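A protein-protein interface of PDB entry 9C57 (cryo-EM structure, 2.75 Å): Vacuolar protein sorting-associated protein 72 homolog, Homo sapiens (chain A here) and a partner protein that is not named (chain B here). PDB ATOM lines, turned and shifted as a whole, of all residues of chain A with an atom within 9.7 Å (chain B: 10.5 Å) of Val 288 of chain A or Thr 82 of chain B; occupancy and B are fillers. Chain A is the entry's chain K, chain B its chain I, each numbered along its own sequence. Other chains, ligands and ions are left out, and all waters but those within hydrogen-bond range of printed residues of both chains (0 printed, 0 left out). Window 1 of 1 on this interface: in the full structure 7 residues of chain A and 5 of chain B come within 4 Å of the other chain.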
ATOM      1  N   PRO A 284      -9.469 -13.101 -33.013  1.00  0.00           N
ATOM      2  CA  PRO A 284      -9.797 -12.177 -31.911  1.00  0.00           C
ATOM      3  C   PRO A 284      -8.993 -10.883 -31.891  1.00  0.00           C
ATOM      4  O   PRO A 284      -9.533  -9.855 -31.465  1.00  0.00           O
ATOM      5  CB  PRO A 284      -9.523 -13.023 -30.661  1.00  0.00           C
ATOM      6  CG  PRO A 284      -9.607 -14.430 -31.120  1.00  0.00           C
ATOM      7  CD  PRO A 284      -9.073 -14.428 -32.509  1.00  0.00           C
ATOM      8  N   LYS A 285      -7.730 -10.885 -32.319  1.00  0.00           N
ATOM      9  CA  LYS A 285      -6.925  -9.660 -32.390  1.00  0.00           C
ATOM     10  C   LYS A 285      -6.731  -9.032 -31.003  1.00  0.00           C
ATOM     11  O   LYS A 285      -7.356  -8.036 -30.638  1.00  0.00           O
ATOM     12  CB  LYS A 285      -7.548  -8.655 -33.367  1.00  0.00           C
ATOM     13  CG  LYS A 285      -6.828  -7.319 -33.413  1.00  0.00           C
ATOM     14  CD  LYS A 285      -7.325  -6.453 -34.559  1.00  0.00           C
ATOM     15  CE  LYS A 285      -6.810  -6.921 -35.915  1.00  0.00           C
ATOM     16  NZ  LYS A 285      -5.473  -7.573 -35.853  1.00  0.00           N
ATOM     17  N   VAL A 286      -5.884  -9.691 -30.218  1.00  0.00           N
ATOM     18  CA  VAL A 286      -5.444  -9.199 -28.911  1.00  0.00           C
ATOM     19  C   VAL A 286      -5.239  -7.687 -28.957  1.00  0.00           C
ATOM     20  O   VAL A 286      -4.663  -7.176 -29.927  1.00  0.00           O
ATOM     21  CB  VAL A 286      -4.151  -9.905 -28.470  1.00  0.00           C
ATOM     22  CG1 VAL A 286      -3.026  -9.633 -29.458  1.00  0.00           C
ATOM     23  CG2 VAL A 286      -3.745  -9.465 -27.079  1.00  0.00           C
ATOM     24  N   PRO A 287      -5.686  -6.925 -27.944  1.00  0.00           N
ATOM     25  CA  PRO A 287      -5.612  -5.462 -28.045  1.00  0.00           C
ATOM     26  C   PRO A 287      -4.203  -4.924 -27.870  1.00  0.00           C
ATOM     27  O   PRO A 287      -3.247  -5.689 -27.723  1.00  0.00           O
ATOM     28  CB  PRO A 287      -6.527  -4.981 -26.907  1.00  0.00           C
ATOM     29  CG  PRO A 287      -7.222  -6.197 -26.393  1.00  0.00           C
ATOM     30  CD  PRO A 287      -6.314  -7.334 -26.680  1.00  0.00           C
ATOM     31  N   VAL A 288      -4.073  -3.605 -27.880  1.00  0.00           N
ATOM     32  CA  VAL A 288      -2.791  -2.949 -27.659  1.00  0.00           C
ATOM     33  C   VAL A 288      -2.689  -2.575 -26.187  1.00  0.00           C
ATOM     34  O   VAL A 288      -3.617  -1.986 -25.620  1.00  0.00           O
ATOM     35  CB  VAL A 288      -2.638  -1.714 -28.565  1.00  0.00           C
ATOM     36  CG1 VAL A 288      -3.828  -0.775 -28.423  1.00  0.00           C
ATOM     37  CG2 VAL A 288      -1.342  -0.985 -28.263  1.00  0.00           C
ATOM     38  N   ARG A 289      -1.575  -2.937 -25.557  1.00  0.00           N
ATOM     39  CA  ARG A 289      -1.336  -2.587 -24.160  1.00  0.00           C
ATOM     40  C   ARG A 289      -0.999  -1.105 -24.122  1.00  0.00           C
ATOM     41  O   ARG A 289       0.153  -0.701 -24.280  1.00  0.00           O
ATOM     42  CB  ARG A 289      -0.219  -3.431 -23.564  1.00  0.00           C
ATOM     43  CG  ARG A 289      -0.566  -4.898 -23.401  1.00  0.00           C
ATOM     44  CD  ARG A 289      -1.423  -5.164 -22.181  1.00  0.00           C
ATOM     45  NE  ARG A 289      -2.844  -5.036 -22.477  1.00  0.00           N
ATOM     46  CZ  ARG A 289      -3.551  -5.927 -23.158  1.00  0.00           C
ATOM     47  NH1 ARG A 289      -2.997  -7.026 -23.643  1.00  0.00           N
ATOM     48  NH2 ARG A 289      -4.846  -5.709 -23.362  1.00  0.00           N
ATOM     49  N   GLU A 290      -2.019  -0.283 -23.912  1.00  0.00           N
ATOM     50  CA  GLU A 290      -1.850   1.155 -24.037  1.00  0.00           C
ATOM     51  C   GLU A 290      -0.997   1.701 -22.898  1.00  0.00           C
ATOM     52  O   GLU A 290      -0.951   1.141 -21.802  1.00  0.00           O
ATOM     53  CB  GLU A 290      -3.214   1.842 -24.058  1.00  0.00           C
ATOM     54  CG  GLU A 290      -3.717   2.246 -25.443  1.00  0.00           C
ATOM     55  CD  GLU A 290      -2.680   2.954 -26.298  1.00  0.00           C
ATOM     56  OE1 GLU A 290      -1.612   3.329 -25.775  1.00  0.00           O
ATOM     57  OE2 GLU A 290      -2.935   3.127 -27.507  1.00  0.00           O
ATOM     58  N   VAL A 291      -0.316   2.811 -23.176  1.00  0.00           N
ATOM     59  CA  VAL A 291       0.614   3.429 -22.241  1.00  0.00           C
ATOM     60  C   VAL A 291       0.273   4.908 -22.110  1.00  0.00           C
ATOM     61  O   VAL A 291      -0.264   5.523 -23.035  1.00  0.00           O
ATOM     62  CB  VAL A 291       2.078   3.231 -22.699  1.00  0.00           C
ATOM     63  CG1 VAL A 291       3.023   4.121 -21.920  1.00  0.00           C
ATOM     64  CG2 VAL A 291       2.482   1.779 -22.549  1.00  0.00           C
ATOM     65  N   PRO A 298       1.022   1.929 -17.566  1.00  0.00           N
ATOM     66  CA  PRO A 298      -0.135   1.365 -18.260  1.00  0.00           C
ATOM     67  C   PRO A 298      -1.320   2.315 -18.183  1.00  0.00           C
ATOM     68  O   PRO A 298      -1.625   2.877 -17.130  1.00  0.00           O
ATOM     69  CB  PRO A 298      -0.400   0.054 -17.507  1.00  0.00           C
ATOM     70  CG  PRO A 298       0.511   0.081 -16.306  1.00  0.00           C
ATOM     71  CD  PRO A 298       1.669   0.912 -16.727  1.00  0.00           C
ATOM     72  N   ALA A 299      -1.981   2.502 -19.317  1.00  0.00           N
ATOM     73  CA  ALA A 299      -3.110   3.413 -19.390  1.00  0.00           C
ATOM     74  C   ALA A 299      -4.347   2.771 -18.785  1.00  0.00           C
ATOM     75  O   ALA A 299      -4.609   1.583 -18.982  1.00  0.00           O
ATOM     76  CB  ALA A 299      -3.384   3.804 -20.841  1.00  0.00           C
ATOM     77  N   LEU A 300      -5.107   3.567 -18.033  1.00  0.00           N
ATOM     78  CA  LEU A 300      -6.399   3.132 -17.522  1.00  0.00           C
ATOM     79  C   LEU A 300      -7.484   4.174 -17.754  1.00  0.00           C
ATOM     80  O   LEU A 300      -8.602   4.003 -17.257  1.00  0.00           O
ATOM     81  CB  LEU A 300      -6.312   2.783 -16.031  1.00  0.00           C
ATOM     82  CG  LEU A 300      -5.644   3.776 -15.083  1.00  0.00           C
ATOM     83  CD1 LEU A 300      -6.150   3.558 -13.671  1.00  0.00           C
ATOM     84  CD2 LEU A 300      -4.133   3.642 -15.122  1.00  0.00           C
ATOM     85  N   ARG A 302      -8.955   7.204 -20.952  1.00  0.00           N
ATOM     86  CA  ARG A 302      -8.854   7.697 -22.322  1.00  0.00           C
ATOM     87  C   ARG A 302      -9.586   9.025 -22.414  1.00  0.00           C
ATOM     88  O   ARG A 302     -10.796   9.085 -22.187  1.00  0.00           O
ATOM     89  CB  ARG A 302      -9.439   6.691 -23.317  1.00  0.00           C
ATOM     90  CG  ARG A 302      -9.242   7.088 -24.764  1.00  0.00           C
ATOM     91  CD  ARG A 302      -9.889   6.111 -25.725  1.00  0.00           C
ATOM     92  NE  ARG A 302      -9.142   4.865 -25.832  1.00  0.00           N
ATOM     93  CZ  ARG A 302      -8.128   4.668 -26.664  1.00  0.00           C
ATOM     94  NH1 ARG A 302      -7.681   5.630 -27.451  1.00  0.00           N
ATOM     95  NH2 ARG A 302      -7.543   3.476 -26.701  1.00  0.00           N
ATOM     96  N   PRO A 309      -4.508   7.938 -24.369  1.00  0.00           N
ATOM     97  CA  PRO A 309      -4.740   7.348 -23.046  1.00  0.00           C
ATOM     98  C   PRO A 309      -3.898   8.024 -21.976  1.00  0.00           C
ATOM     99  O   PRO A 309      -2.915   8.712 -22.257  1.00  0.00           O
ATOM    100  CB  PRO A 309      -4.327   5.883 -23.226  1.00  0.00           C
ATOM    101  CG  PRO A 309      -4.211   5.671 -24.690  1.00  0.00           C
ATOM    102  CD  PRO A 309      -3.844   6.987 -25.272  1.00  0.00           C
ATOM    103  N   ASP B  75      10.423  -9.922 -27.011  1.00  0.00           N
ATOM    104  CA  ASP B  75       9.385  -8.936 -26.759  1.00  0.00           C
ATOM    105  C   ASP B  75       8.205  -9.114 -27.697  1.00  0.00           C
ATOM    106  O   ASP B  75       7.051  -9.063 -27.259  1.00  0.00           O
ATOM    107  CB  ASP B  75       9.960  -7.523 -26.915  1.00  0.00           C
ATOM    108  CG  ASP B  75      10.693  -7.054 -25.683  1.00  0.00           C
ATOM    109  OD1 ASP B  75      10.280  -7.425 -24.565  1.00  0.00           O
ATOM    110  OD2 ASP B  75      11.684  -6.313 -25.832  1.00  0.00           O
ATOM    111  N   THR B  76       8.470  -9.349 -28.978  1.00  0.00           N
ATOM    112  CA  THR B  76       7.433  -9.427 -30.001  1.00  0.00           C
ATOM    113  C   THR B  76       6.815 -10.807 -30.091  1.00  0.00           C
ATOM    114  O   THR B  76       6.265 -11.180 -31.129  1.00  0.00           O
ATOM    115  CB  THR B  76       8.008  -9.008 -31.346  1.00  0.00           C
ATOM    116  OG1 THR B  76       9.155  -9.813 -31.638  1.00  0.00           O
ATOM    117  CG2 THR B  76       8.400  -7.543 -31.314  1.00  0.00           C
ATOM    118  N   GLY B  77       6.884 -11.590 -29.021  1.00  0.00           N
ATOM    119  CA  GLY B  77       5.909 -12.643 -28.856  1.00  0.00           C
ATOM    120  C   GLY B  77       4.570 -11.950 -28.944  1.00  0.00           C
ATOM    121  O   GLY B  77       4.523 -10.719 -28.878  1.00  0.00           O
ATOM    122  N   GLN B  78       3.475 -12.687 -29.063  1.00  0.00           N
ATOM    123  CA  GLN B  78       2.256 -12.047 -29.533  1.00  0.00           C
ATOM    124  C   GLN B  78       2.586 -11.427 -30.890  1.00  0.00           C
ATOM    125  O   GLN B  78       3.134 -12.130 -31.746  1.00  0.00           O
ATOM    126  CB  GLN B  78       1.738 -11.039 -28.503  1.00  0.00           C
ATOM    127  CG  GLN B  78       1.146 -11.699 -27.258  1.00  0.00           C
ATOM    128  CD  GLN B  78       2.180 -12.410 -26.402  1.00  0.00           C
ATOM    129  OE1 GLN B  78       3.086 -13.060 -26.917  1.00  0.00           O
ATOM    130  NE2 GLN B  78       2.041 -12.297 -25.088  1.00  0.00           N
ATOM    131  N   GLY B  79       2.280 -10.150 -31.135  1.00  0.00           N
ATOM    132  CA  GLY B  79       2.358  -9.684 -32.511  1.00  0.00           C
ATOM    133  C   GLY B  79       2.750  -8.257 -32.852  1.00  0.00           C
ATOM    134  O   GLY B  79       2.413  -7.799 -33.947  1.00  0.00           O
ATOM    135  N   TYR B  80       3.456  -7.540 -31.981  1.00  0.00           N
ATOM    136  CA  TYR B  80       3.639  -6.105 -32.195  1.00  0.00           C
ATOM    137  C   TYR B  80       2.296  -5.457 -32.510  1.00  0.00           C
ATOM    138  O   TYR B  80       2.173  -4.631 -33.415  1.00  0.00           O
ATOM    139  CB  TYR B  80       4.659  -5.809 -33.305  1.00  0.00           C
ATOM    140  CG  TYR B  80       4.812  -4.321 -33.573  1.00  0.00           C
ATOM    141  CD1 TYR B  80       5.529  -3.505 -32.716  1.00  0.00           C
ATOM    142  CD2 TYR B  80       4.229  -3.737 -34.691  1.00  0.00           C
ATOM    143  CE1 TYR B  80       5.645  -2.147 -32.957  1.00  0.00           C
ATOM    144  CE2 TYR B  80       4.336  -2.391 -34.934  1.00  0.00           C
ATOM    145  CZ  TYR B  80       5.047  -1.601 -34.072  1.00  0.00           C
ATOM    146  OH  TYR B  80       5.150  -0.259 -34.332  1.00  0.00           O
ATOM    147  N   ARG B  81       1.267  -5.854 -31.787  1.00  0.00           N
ATOM    148  CA  ARG B  81       0.052  -5.062 -31.756  1.00  0.00           C
ATOM    149  C   ARG B  81      -0.238  -4.818 -30.288  1.00  0.00           C
ATOM    150  O   ARG B  81      -0.872  -3.827 -29.914  1.00  0.00           O
ATOM    151  CB  ARG B  81      -1.087  -5.779 -32.478  1.00  0.00           C
ATOM    152  CG  ARG B  81      -2.455  -5.230 -32.166  1.00  0.00           C
ATOM    153  CD  ARG B  81      -3.374  -5.333 -33.365  1.00  0.00           C
ATOM    154  NE  ARG B  81      -4.361  -4.265 -33.369  1.00  0.00           N
ATOM    155  CZ  ARG B  81      -5.324  -4.134 -32.470  1.00  0.00           C
ATOM    156  NH1 ARG B  81      -5.472  -5.004 -31.485  1.00  0.00           N
ATOM    157  NH2 ARG B  81      -6.162  -3.106 -32.561  1.00  0.00           N
ATOM    158  N   THR B  82       0.250  -5.733 -29.451  1.00  0.00           N
ATOM    159  CA  THR B  82       0.272  -5.521 -28.012  1.00  0.00           C
ATOM    160  C   THR B  82       1.273  -4.434 -27.634  1.00  0.00           C
ATOM    161  O   THR B  82       0.945  -3.498 -26.899  1.00  0.00           O
ATOM    162  CB  THR B  82       0.622  -6.838 -27.320  1.00  0.00           C
ATOM    163  OG1 THR B  82       0.064  -7.928 -28.062  1.00  0.00           O
ATOM    164  CG2 THR B  82       0.086  -6.866 -25.911  1.00  0.00           C
ATOM    165  N   VAL B  83       2.498  -4.532 -28.149  1.00  0.00           N
ATOM    166  CA  VAL B  83       3.612  -3.741 -27.635  1.00  0.00           C
ATOM    167  C   VAL B  83       3.832  -2.511 -28.503  1.00  0.00           C
ATOM    168  O   VAL B  83       4.786  -1.756 -28.292  1.00  0.00           O
ATOM    169  CB  VAL B  83       4.906  -4.575 -27.543  1.00  0.00           C
ATOM    170  CG1 VAL B  83       4.921  -5.387 -26.261  1.00  0.00           C
ATOM    171  CG2 VAL B  83       5.072  -5.473 -28.755  1.00  0.00           C
ATOM    172  N   LYS B  84       2.949  -2.294 -29.477  1.00  0.00           N
ATOM    173  CA  LYS B  84       3.045  -1.103 -30.311  1.00  0.00           C
ATOM    174  C   LYS B  84       3.199   0.153 -29.465  1.00  0.00           C
ATOM    175  O   LYS B  84       4.074   0.985 -29.734  1.00  0.00           O
ATOM    176  CB  LYS B  84       1.801  -1.015 -31.197  1.00  0.00           C
ATOM    177  CG  LYS B  84       1.512   0.348 -31.783  1.00  0.00           C
ATOM    178  CD  LYS B  84       0.865   0.230 -33.154  1.00  0.00           C
ATOM    179  CE  LYS B  84      -0.457  -0.519 -33.092  1.00  0.00           C
ATOM    180  NZ  LYS B  84      -1.524   0.277 -32.436  1.00  0.00           N
ATOM    181  N   ALA B  85       2.383   0.291 -28.424  1.00  0.00           N
ATOM    182  CA  ALA B  85       2.440   1.435 -27.527  1.00  0.00           C
ATOM    183  C   ALA B  85       3.681   1.466 -26.651  1.00  0.00           C
ATOM    184  O   ALA B  85       4.279   2.531 -26.496  1.00  0.00           O
ATOM    185  CB  ALA B  85       1.203   1.458 -26.623  1.00  0.00           C
ATOM    186  N   LYS B  86       4.083   0.332 -26.075  1.00  0.00           N
ATOM    187  CA  LYS B  86       5.245   0.332 -25.195  1.00  0.00           C
ATOM    188  C   LYS B  86       6.527   0.653 -25.945  1.00  0.00           C
ATOM    189  O   LYS B  86       7.478   1.153 -25.338  1.00  0.00           O
ATOM    190  CB  LYS B  86       5.370  -1.018 -24.486  1.00  0.00           C
ATOM    191  CG  LYS B  86       6.475  -1.059 -23.432  1.00  0.00           C
ATOM    192  CD  LYS B  86       6.662  -2.434 -22.789  1.00  0.00           C
ATOM    193  CE  LYS B  86       5.359  -3.197 -22.601  1.00  0.00           C
ATOM    194  NZ  LYS B  86       4.356  -2.428 -21.812  1.00  0.00           N
ATOM    195  N   LEU B  87       6.577   0.383 -27.246  1.00  0.00           N
ATOM    196  CA  LEU B  87       7.741   0.715 -28.053  1.00  0.00           C
ATOM    197  C   LEU B  87       7.662   2.102 -28.670  1.00  0.00           C
ATOM    198  O   LEU B  87       8.681   2.796 -28.730  1.00  0.00           O
ATOM    199  CB  LEU B  87       7.927  -0.316 -29.171  1.00  0.00           C
ATOM    200  CG  LEU B  87       7.966  -1.785 -28.746  1.00  0.00           C
ATOM    201  CD1 LEU B  87       8.244  -2.672 -29.941  1.00  0.00           C
ATOM    202  CD2 LEU B  87       9.000  -2.015 -27.662  1.00  0.00           C
ATOM    203  N   GLY B  88       6.485   2.529 -29.115  1.00  0.00           N
ATOM    204  CA  GLY B  88       6.363   3.811 -29.779  1.00  0.00           C
ATOM    205  C   GLY B  88       6.620   4.988 -28.864  1.00  0.00           C
ATOM    206  O   GLY B  88       7.038   6.057 -29.319  1.00  0.00           O
ATOM    207  N   SER B  89       6.377   4.804 -27.569  1.00  0.00           N
ATOM    208  CA  SER B  89       6.498   5.894 -26.611  1.00  0.00           C
ATOM    209  C   SER B  89       7.927   6.124 -26.142  1.00  0.00           C
ATOM    210  O   SER B  89       8.171   7.102 -25.427  1.00  0.00           O
ATOM    211  CB  SER B  89       5.603   5.618 -25.404  1.00  0.00           C
ATOM    212  OG  SER B  89       5.796   4.302 -24.922  1.00  0.00           O
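O of Ala 85 of chain B lies within hydrogen-bond range of OG of Ser 89 of chain B. The backbone NH (N) of Ala 299 of chain A lies within hydrogen-bond range of the backbone carbonyl oxygen (O) of Glu 290 of chain A, 3.0 Å away.
NH1 of Arg 81 of chain B is in hydrogen-bond range of O of Val 286 of chain A (2.8 Å). O of Thr 82 of chain B is in hydrogen-bond range of N of Arg 289 of chain A.
Along chain A the printed residues that touch a printed residue of chain B span positions 285 to 290. Among the printed residues, no Asp or Glu carboxylate lies within 4 Å of a Lys or Arg side-chain nitrogen of the other chain.
Printed residues of chain B within 4 Å of Lys 285 of chain A: Arg 81. Printed residues of chain B within 4 Å of Val 286 of chain A: Arg 81 and Thr 82. Pro 287 of chain A touches just these residues of chain B: Arg 81 and Thr 82. Val 288 of chain A touches just these residues of chain B: Arg 81 (3.1 Å), Thr 82 (3.7 Å) and Ala 85 (3.9 Å). Of chain B, only Thr 82 and Ala 85 come within 4 Å of Arg 289 of chain A. Glu 290 of chain A touches just one residue of chain B: Ala 85. Gln 78 of chain B touches none of the printed residues of chain A. No residue of chain A comes within 4 Å of Gly 79 of chain B. Arg 81 of chain B touches four residues of chain A. Thr 82 of chain B touches just these residues of chain A: Val 286, Pro 287, Val 288 and Arg 289. No residue of chain A comes within 4 Å of Val 83 of chain B. Of the printed residues of chain A, Ala 85 of chain B touches Val 288, Arg 289 and Glu 290. The nearest printed residue of chain A that does not touch Ala 85 of chain B is Val 291 of chain A (4.002 Å).
Among the printed residues, merely in contact across the chains: Lys 285 of chain A with Arg 81 of chain B, Val 286 of chain A with Thr 82 of chain B, Pro 287 of chain A with Arg 81 of chain B, Pro 287 of chain A with Thr 82 of chain B, Val 288 of chain A with Arg 81 of chain B, Val 288 of chain A with Thr 82 of chain B, Val 288 of chain A with Ala 85 of chain B, Arg 289 of chain A with Ala 85 of chain B and Glu 290 of chain A with Ala 85 of chain B.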
